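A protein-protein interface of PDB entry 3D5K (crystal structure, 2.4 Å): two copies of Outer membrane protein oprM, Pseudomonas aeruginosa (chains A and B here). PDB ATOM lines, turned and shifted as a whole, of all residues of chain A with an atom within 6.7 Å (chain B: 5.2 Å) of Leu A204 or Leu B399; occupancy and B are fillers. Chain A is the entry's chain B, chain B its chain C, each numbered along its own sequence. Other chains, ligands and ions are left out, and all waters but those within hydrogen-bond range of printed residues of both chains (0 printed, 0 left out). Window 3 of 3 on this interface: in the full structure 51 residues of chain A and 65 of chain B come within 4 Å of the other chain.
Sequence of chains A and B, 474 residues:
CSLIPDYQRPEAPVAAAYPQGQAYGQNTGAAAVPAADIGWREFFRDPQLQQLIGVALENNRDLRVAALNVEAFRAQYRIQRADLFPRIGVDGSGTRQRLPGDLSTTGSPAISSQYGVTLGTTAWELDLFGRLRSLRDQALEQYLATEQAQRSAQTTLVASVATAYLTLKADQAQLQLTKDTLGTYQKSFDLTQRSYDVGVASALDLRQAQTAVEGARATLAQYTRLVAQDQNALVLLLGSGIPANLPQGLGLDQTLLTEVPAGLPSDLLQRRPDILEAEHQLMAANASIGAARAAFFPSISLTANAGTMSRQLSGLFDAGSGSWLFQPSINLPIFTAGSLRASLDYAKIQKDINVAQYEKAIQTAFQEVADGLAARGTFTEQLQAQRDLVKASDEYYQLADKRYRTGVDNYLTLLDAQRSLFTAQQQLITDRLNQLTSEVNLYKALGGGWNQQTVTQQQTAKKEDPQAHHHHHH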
ATOM      1  N   TYR A 196       3.657  18.878   1.412  1.00  0.00           N
ATOM      2  CA  TYR A 196       3.760  20.242   0.887  1.00  0.00           C
ATOM      3  C   TYR A 196       2.801  20.443  -0.289  1.00  0.00           C
ATOM      4  O   TYR A 196       2.197  21.511  -0.438  1.00  0.00           O
ATOM      5  CB  TYR A 196       5.203  20.550   0.455  1.00  0.00           C
ATOM      6  CG  TYR A 196       5.364  21.854  -0.304  1.00  0.00           C
ATOM      7  CD1 TYR A 196       5.556  23.059   0.374  1.00  0.00           C
ATOM      8  CD2 TYR A 196       5.316  21.884  -1.698  1.00  0.00           C
ATOM      9  CE1 TYR A 196       5.694  24.261  -0.319  1.00  0.00           C
ATOM     10  CE2 TYR A 196       5.456  23.083  -2.400  1.00  0.00           C
ATOM     11  CZ  TYR A 196       5.646  24.265  -1.704  1.00  0.00           C
ATOM     12  OH  TYR A 196       5.786  25.449  -2.392  1.00  0.00           O
ATOM     13  N   ALA A 201       2.649  20.780   4.820  1.00  0.00           N
ATOM     14  CA  ALA A 201       4.064  21.100   5.028  1.00  0.00           C
ATOM     15  C   ALA A 201       4.454  22.403   4.327  1.00  0.00           C
ATOM     16  O   ALA A 201       3.986  22.686   3.216  1.00  0.00           O
ATOM     17  CB  ALA A 201       4.950  19.956   4.553  1.00  0.00           C
ATOM     18  N   SER A 202       5.309  23.186   4.985  1.00  0.00           N
ATOM     19  CA  SER A 202       5.788  24.456   4.438  1.00  0.00           C
ATOM     20  C   SER A 202       7.022  24.267   3.550  1.00  0.00           C
ATOM     21  O   SER A 202       7.677  23.221   3.598  1.00  0.00           O
ATOM     22  CB  SER A 202       6.080  25.456   5.565  1.00  0.00           C
ATOM     23  OG  SER A 202       7.283  25.143   6.250  1.00  0.00           O
ATOM     24  N   ALA A 203       7.328  25.281   2.741  1.00  0.00           N
ATOM     25  CA  ALA A 203       8.527  25.276   1.903  1.00  0.00           C
ATOM     26  C   ALA A 203       9.802  25.131   2.737  1.00  0.00           C
ATOM     27  O   ALA A 203      10.763  24.499   2.302  1.00  0.00           O
ATOM     28  CB  ALA A 203       8.588  26.534   1.053  1.00  0.00           C
ATOM     29  N   LEU A 204       9.793  25.714   3.937  1.00  0.00           N
ATOM     30  CA  LEU A 204      10.902  25.606   4.882  1.00  0.00           C
ATOM     31  C   LEU A 204      11.128  24.159   5.327  1.00  0.00           C
ATOM     32  O   LEU A 204      12.265  23.688   5.357  1.00  0.00           O
ATOM     33  CB  LEU A 204      10.652  26.497   6.102  1.00  0.00           C
ATOM     34  CG  LEU A 204      11.771  26.575   7.144  1.00  0.00           C
ATOM     35  CD1 LEU A 204      12.792  27.647   6.769  1.00  0.00           C
ATOM     36  CD2 LEU A 204      11.187  26.845   8.521  1.00  0.00           C
ATOM     37  N   ASP A 205      10.042  23.468   5.675  1.00  0.00           N
ATOM     38  CA  ASP A 205      10.098  22.050   6.045  1.00  0.00           C
ATOM     39  C   ASP A 205      10.797  21.218   4.971  1.00  0.00           C
ATOM     40  O   ASP A 205      11.630  20.365   5.283  1.00  0.00           O
ATOM     41  CB  ASP A 205       8.686  21.490   6.281  1.00  0.00           C
ATOM     42  CG  ASP A 205       7.986  22.117   7.483  1.00  0.00           C
ATOM     43  OD1 ASP A 205       8.644  22.797   8.301  1.00  0.00           O
ATOM     44  OD2 ASP A 205       6.758  21.920   7.613  1.00  0.00           O
ATOM     45  N   LEU A 206      10.453  21.492   3.713  1.00  0.00           N
ATOM     46  CA  LEU A 206      10.930  20.725   2.567  1.00  0.00           C
ATOM     47  C   LEU A 206      12.427  20.891   2.344  1.00  0.00           C
ATOM     48  O   LEU A 206      13.137  19.923   2.073  1.00  0.00           O
ATOM     49  CB  LEU A 206      10.156  21.130   1.307  1.00  0.00           C
ATOM     50  CG  LEU A 206      10.390  20.337   0.021  1.00  0.00           C
ATOM     51  CD1 LEU A 206       9.735  18.963   0.096  1.00  0.00           C
ATOM     52  CD2 LEU A 206       9.874  21.118  -1.179  1.00  0.00           C
ATOM     53  N   ARG A 207      12.902  22.124   2.464  1.00  0.00           N
ATOM     54  CA  ARG A 207      14.317  22.422   2.272  1.00  0.00           C
ATOM     55  C   ARG A 207      15.175  21.984   3.456  1.00  0.00           C
ATOM     56  O   ARG A 207      16.362  21.718   3.290  1.00  0.00           O
ATOM     57  CB  ARG A 207      14.511  23.899   1.927  1.00  0.00           C
ATOM     58  CG  ARG A 207      13.704  24.290   0.699  1.00  0.00           C
ATOM     59  CD  ARG A 207      14.283  25.465  -0.037  1.00  0.00           C
ATOM     60  NE  ARG A 207      13.657  25.623  -1.348  1.00  0.00           N
ATOM     61  CZ  ARG A 207      14.106  25.071  -2.474  1.00  0.00           C
ATOM     62  NH1 ARG A 207      15.197  24.311  -2.472  1.00  0.00           N
ATOM     63  NH2 ARG A 207      13.457  25.283  -3.614  1.00  0.00           N
ATOM     64  N   GLN A 208      14.565  21.896   4.639  1.00  0.00           N
ATOM     65  CA  GLN A 208      15.214  21.320   5.820  1.00  0.00           C
ATOM     66  C   GLN A 208      15.464  19.827   5.619  1.00  0.00           C
ATOM     67  O   GLN A 208      16.555  19.332   5.891  1.00  0.00           O
ATOM     68  CB  GLN A 208      14.359  21.536   7.069  1.00  0.00           C
ATOM     69  CG  GLN A 208      14.535  22.894   7.728  1.00  0.00           C
ATOM     70  CD  GLN A 208      13.653  23.074   8.956  1.00  0.00           C
ATOM     71  OE1 GLN A 208      12.459  22.782   8.928  1.00  0.00           O
ATOM     72  NE2 GLN A 208      14.242  23.567  10.036  1.00  0.00           N
ATOM     73  N   ALA A 209      14.441  19.128   5.126  1.00  0.00           N
ATOM     74  CA  ALA A 209      14.534  17.714   4.763  1.00  0.00           C
ATOM     75  C   ALA A 209      15.573  17.456   3.675  1.00  0.00           C
ATOM     76  O   ALA A 209      16.214  16.404   3.665  1.00  0.00           O
ATOM     77  CB  ALA A 209      13.174  17.194   4.323  1.00  0.00           C
ATOM     78  N   TYR A 411       9.391  21.119  11.954  1.00  0.00           N
ATOM     79  CA  TYR A 411      10.337  20.162  11.375  1.00  0.00           C
ATOM     80  C   TYR A 411      11.738  20.266  11.989  1.00  0.00           C
ATOM     81  O   TYR A 411      12.525  19.325  11.897  1.00  0.00           O
ATOM     82  CB  TYR A 411      10.400  20.309   9.843  1.00  0.00           C
ATOM     83  CG  TYR A 411      11.045  19.129   9.147  1.00  0.00           C
ATOM     84  CD1 TYR A 411      10.282  18.035   8.732  1.00  0.00           C
ATOM     85  CD2 TYR A 411      12.421  19.097   8.917  1.00  0.00           C
ATOM     86  CE1 TYR A 411      10.878  16.941   8.103  1.00  0.00           C
ATOM     87  CE2 TYR A 411      13.025  18.011   8.298  1.00  0.00           C
ATOM     88  CZ  TYR A 411      12.251  16.938   7.893  1.00  0.00           C
ATOM     89  OH  TYR A 411      12.860  15.866   7.283  1.00  0.00           O
ATOM     90  N   GLU B 395      19.036  28.319   0.303  1.00  0.00           N
ATOM     91  CA  GLU B 395      17.579  28.447   0.188  1.00  0.00           C
ATOM     92  C   GLU B 395      16.908  28.358   1.565  1.00  0.00           C
ATOM     93  O   GLU B 395      15.944  29.075   1.839  1.00  0.00           O
ATOM     94  CB  GLU B 395      16.999  27.368  -0.741  1.00  0.00           C
ATOM     95  CG  GLU B 395      17.613  27.286  -2.147  1.00  0.00           C
ATOM     96  CD  GLU B 395      16.833  28.044  -3.225  1.00  0.00           C
ATOM     97  OE1 GLU B 395      16.009  28.928  -2.893  1.00  0.00           O
ATOM     98  OE2 GLU B 395      17.049  27.748  -4.423  1.00  0.00           O
ATOM     99  N   TYR B 396      17.426  27.473   2.417  1.00  0.00           N
ATOM    100  CA  TYR B 396      16.938  27.295   3.791  1.00  0.00           C
ATOM    101  C   TYR B 396      17.123  28.563   4.632  1.00  0.00           C
ATOM    102  O   TYR B 396      16.207  28.969   5.350  1.00  0.00           O
ATOM    103  CB  TYR B 396      17.608  26.064   4.442  1.00  0.00           C
ATOM    104  CG  TYR B 396      17.368  25.855   5.934  1.00  0.00           C
ATOM    105  CD1 TYR B 396      16.162  26.216   6.538  1.00  0.00           C
ATOM    106  CD2 TYR B 396      18.343  25.256   6.735  1.00  0.00           C
ATOM    107  CE1 TYR B 396      15.950  26.026   7.902  1.00  0.00           C
ATOM    108  CE2 TYR B 396      18.135  25.052   8.102  1.00  0.00           C
ATOM    109  CZ  TYR B 396      16.935  25.439   8.675  1.00  0.00           C
ATOM    110  OH  TYR B 396      16.713  25.242  10.018  1.00  0.00           O
ATOM    111  N   TYR B 397      18.297  29.184   4.525  1.00  0.00           N
ATOM    112  CA  TYR B 397      18.591  30.442   5.215  1.00  0.00           C
ATOM    113  C   TYR B 397      17.671  31.590   4.783  1.00  0.00           C
ATOM    114  O   TYR B 397      17.201  32.363   5.621  1.00  0.00           O
ATOM    115  CB  TYR B 397      20.064  30.835   5.019  1.00  0.00           C
ATOM    116  CG  TYR B 397      20.379  32.259   5.435  1.00  0.00           C
ATOM    117  CD1 TYR B 397      20.495  32.603   6.784  1.00  0.00           C
ATOM    118  CD2 TYR B 397      20.553  33.262   4.481  1.00  0.00           C
ATOM    119  CE1 TYR B 397      20.776  33.907   7.172  1.00  0.00           C
ATOM    120  CE2 TYR B 397      20.832  34.576   4.858  1.00  0.00           C
ATOM    121  CZ  TYR B 397      20.942  34.889   6.207  1.00  0.00           C
ATOM    122  OH  TYR B 397      21.218  36.182   6.592  1.00  0.00           O
ATOM    123  N   GLN B 398      17.420  31.694   3.479  1.00  0.00           N
ATOM    124  CA  GLN B 398      16.639  32.803   2.926  1.00  0.00           C
ATOM    125  C   GLN B 398      15.190  32.787   3.408  1.00  0.00           C
ATOM    126  O   GLN B 398      14.639  33.830   3.758  1.00  0.00           O
ATOM    127  CB  GLN B 398      16.716  32.813   1.398  1.00  0.00           C
ATOM    128  CG  GLN B 398      18.066  33.273   0.866  1.00  0.00           C
ATOM    129  CD  GLN B 398      18.249  32.991  -0.614  1.00  0.00           C
ATOM    130  OE1 GLN B 398      17.861  31.929  -1.116  1.00  0.00           O
ATOM    131  NE2 GLN B 398      18.858  33.939  -1.321  1.00  0.00           N
ATOM    132  N   LEU B 399      14.589  31.599   3.436  1.00  0.00           N
ATOM    133  CA  LEU B 399      13.242  31.423   3.971  1.00  0.00           C
ATOM    134  C   LEU B 399      13.196  31.668   5.481  1.00  0.00           C
ATOM    135  O   LEU B 399      12.250  32.277   5.983  1.00  0.00           O
ATOM    136  CB  LEU B 399      12.709  30.026   3.649  1.00  0.00           C
ATOM    137  CG  LEU B 399      12.557  29.635   2.173  1.00  0.00           C
ATOM    138  CD1 LEU B 399      12.456  28.120   2.028  1.00  0.00           C
ATOM    139  CD2 LEU B 399      11.366  30.325   1.526  1.00  0.00           C
ATOM    140  N   ALA B 400      14.221  31.196   6.192  1.00  0.00           N
ATOM    141  CA  ALA B 400      14.315  31.356   7.645  1.00  0.00           C
ATOM    142  C   ALA B 400      14.453  32.821   8.063  1.00  0.00           C
ATOM    143  O   ALA B 400      13.815  33.257   9.022  1.00  0.00           O
ATOM    144  CB  ALA B 400      15.469  30.528   8.202  1.00  0.00           C
ATOM    145  N   ASP B 401      15.281  33.574   7.337  1.00  0.00           N
ATOM    146  CA  ASP B 401      15.470  35.004   7.598  1.00  0.00           C
ATOM    147  C   ASP B 401      14.173  35.775   7.379  1.00  0.00           C
ATOM    148  O   ASP B 401      13.840  36.676   8.149  1.00  0.00           O
ATOM    149  CB  ASP B 401      16.585  35.579   6.717  1.00  0.00           C
ATOM    150  CG  ASP B 401      16.960  37.009   7.097  1.00  0.00           C
ATOM    151  OD1 ASP B 401      17.273  37.262   8.285  1.00  0.00           O
ATOM    152  OD2 ASP B 401      16.949  37.884   6.204  1.00  0.00           O
ATOM    153  N   LYS B 402      13.448  35.393   6.329  1.00  0.00           N
ATOM    154  CA  LYS B 402      12.178  36.008   5.966  1.00  0.00           C
ATOM    155  C   LYS B 402      11.071  35.712   6.981  1.00  0.00           C
ATOM    156  O   LYS B 402      10.245  36.578   7.260  1.00  0.00           O
ATOM    157  CB  LYS B 402      11.761  35.545   4.569  1.00  0.00           C
ATOM    158  CG  LYS B 402      10.692  36.393   3.900  1.00  0.00           C
ATOM    159  CD  LYS B 402      10.454  35.962   2.454  1.00  0.00           C
ATOM    160  CE  LYS B 402       9.678  34.645   2.358  1.00  0.00           C
ATOM    161  NZ  LYS B 402       9.366  34.275   0.940  1.00  0.00           N
ATOM    162  N   ARG B 403      11.054  34.500   7.527  1.00  0.00           N
ATOM    163  CA  ARG B 403      10.010  34.109   8.486  1.00  0.00           C
ATOM    164  C   ARG B 403      10.244  34.656   9.895  1.00  0.00           C
ATOM    165  O   ARG B 403       9.293  34.813  10.663  1.00  0.00           O
ATOM    166  CB  ARG B 403       9.822  32.589   8.524  1.00  0.00           C
ATOM    167  CG  ARG B 403       9.319  31.993   7.219  1.00  0.00           C
ATOM    168  CD  ARG B 403       9.032  30.513   7.365  1.00  0.00           C
ATOM    169  NE  ARG B 403       7.644  30.276   7.749  1.00  0.00           N
ATOM    170  CZ  ARG B 403       7.206  29.178   8.357  1.00  0.00           C
ATOM    171  NH1 ARG B 403       8.047  28.202   8.674  1.00  0.00           N
ATOM    172  NH2 ARG B 403       5.922  29.062   8.659  1.00  0.00           N
ATOM    173  N   TYR B 404      11.499  34.938  10.241  1.00  0.00           N
ATOM    174  CA  TYR B 404      11.784  35.589  11.517  1.00  0.00           C
ATOM    175  C   TYR B 404      11.343  37.062  11.524  1.00  0.00           C
ATOM    176  O   TYR B 404      10.618  37.486  12.429  1.00  0.00           O
ATOM    177  CB  TYR B 404      13.258  35.461  11.944  1.00  0.00           C
ATOM    178  CG  TYR B 404      13.544  36.300  13.176  1.00  0.00           C
ATOM    179  CD1 TYR B 404      13.080  35.905  14.432  1.00  0.00           C
ATOM    180  CD2 TYR B 404      14.224  37.514  13.077  1.00  0.00           C
ATOM    181  CE1 TYR B 404      13.306  36.682  15.556  1.00  0.00           C
ATOM    182  CE2 TYR B 404      14.456  38.299  14.198  1.00  0.00           C
ATOM    183  CZ  TYR B 404      13.995  37.877  15.433  1.00  0.00           C
ATOM    184  OH  TYR B 404      14.220  38.650  16.549  1.00  0.00           O
ATOM    185  N   ASP B 409       8.212  32.448  12.595  1.00  0.00           N
ATOM    186  CA  ASP B 409       9.087  31.478  13.245  1.00  0.00           C
ATOM    187  C   ASP B 409       9.939  32.113  14.349  1.00  0.00           C
ATOM    188  O   ASP B 409       9.998  33.340  14.478  1.00  0.00           O
ATOM    189  CB  ASP B 409       9.993  30.806  12.203  1.00  0.00           C
ATOM    190  CG  ASP B 409       9.338  29.600  11.539  1.00  0.00           C
ATOM    191  OD1 ASP B 409       8.093  29.577  11.397  1.00  0.00           O
ATOM    192  OD2 ASP B 409      10.077  28.669  11.149  1.00  0.00           O
ATOM    193  N   THR B 413      15.452  28.786  14.363  1.00  0.00           N
ATOM    194  CA  THR B 413      15.442  28.323  12.974  1.00  0.00           C
ATOM    195  C   THR B 413      16.460  29.083  12.121  1.00  0.00           C
ATOM    196  O   THR B 413      17.219  28.470  11.361  1.00  0.00           O
ATOM    197  CB  THR B 413      14.025  28.422  12.353  1.00  0.00           C
ATOM    198  OG1 THR B 413      13.107  27.646  13.132  1.00  0.00           O
ATOM    199  CG2 THR B 413      14.015  27.907  10.925  1.00  0.00           C
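No position is printed for both chains.
NE2 of Gln A208 sits at hydrogen-bond distance from OH of Tyr B396, at 3.0 Å.
Of the 11 printed residues of chain A, 4 touch a printed residue of chain B. Hydrophobic or aromatic side chains of chain A within 4 Å of the printed part of chain B: Leu A204. Among the printed residues, 10 pairs touch across the chains.
The side-chain hydroxyl of Ser A202 sits close to the backbone NH of Leu A204. The side-chain carboxylate (OD2) of Asp A205 lies within hydrogen-bond range of the backbone NH (N) of Ser A202, 3.3 Å away. NH1 of Arg B403 lies within salt-bridge range of OD1 of Asp B409 (3.1 Å).
Leu A204 touches just these residues of chain B: Tyr B396 (3.7 Å), Leu B399 (3.9 Å), Ala B400 (3.9 Å), Arg B403 (3.4 Å), Asp B409 (3.4 Å) and Thr B413 (3.9 Å). Asp A205 touches none of the printed residues of chain B. Printed residues of chain B within 4 Å of Gln A208: Tyr B396. Tyr A411 touches none of the printed residues of chain B. Of the printed residues of chain A, Glu B395 touches Arg A207. Of the printed residues of chain A, Leu B399 touches Leu A204 and Arg A207. Printed residues of chain A within 4 Å of Arg B403: Ser A202 and Leu A204. The nearest printed residue of chain B that does not touch Leu A204 is Glu B395 (6.0 Å). The nearest printed residue of chain A that does not touch Leu B399 is Ala A203 (4.01 Å). The nearest printed residue of chain A that does not touch Asp B409 is Ser A202 (6.7 Å).
Among the printed residues, pairs that only touch across the chains: Ser A202 with Arg B403, Leu A204 with Tyr B396, Leu A204 with Leu B399, Leu A204 with Ala B400, Leu A204 with Arg B403, Leu A204 with Asp B409, Leu A204 with Thr B413, Arg A207 with Glu B395 and Arg A207 with Leu B399.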
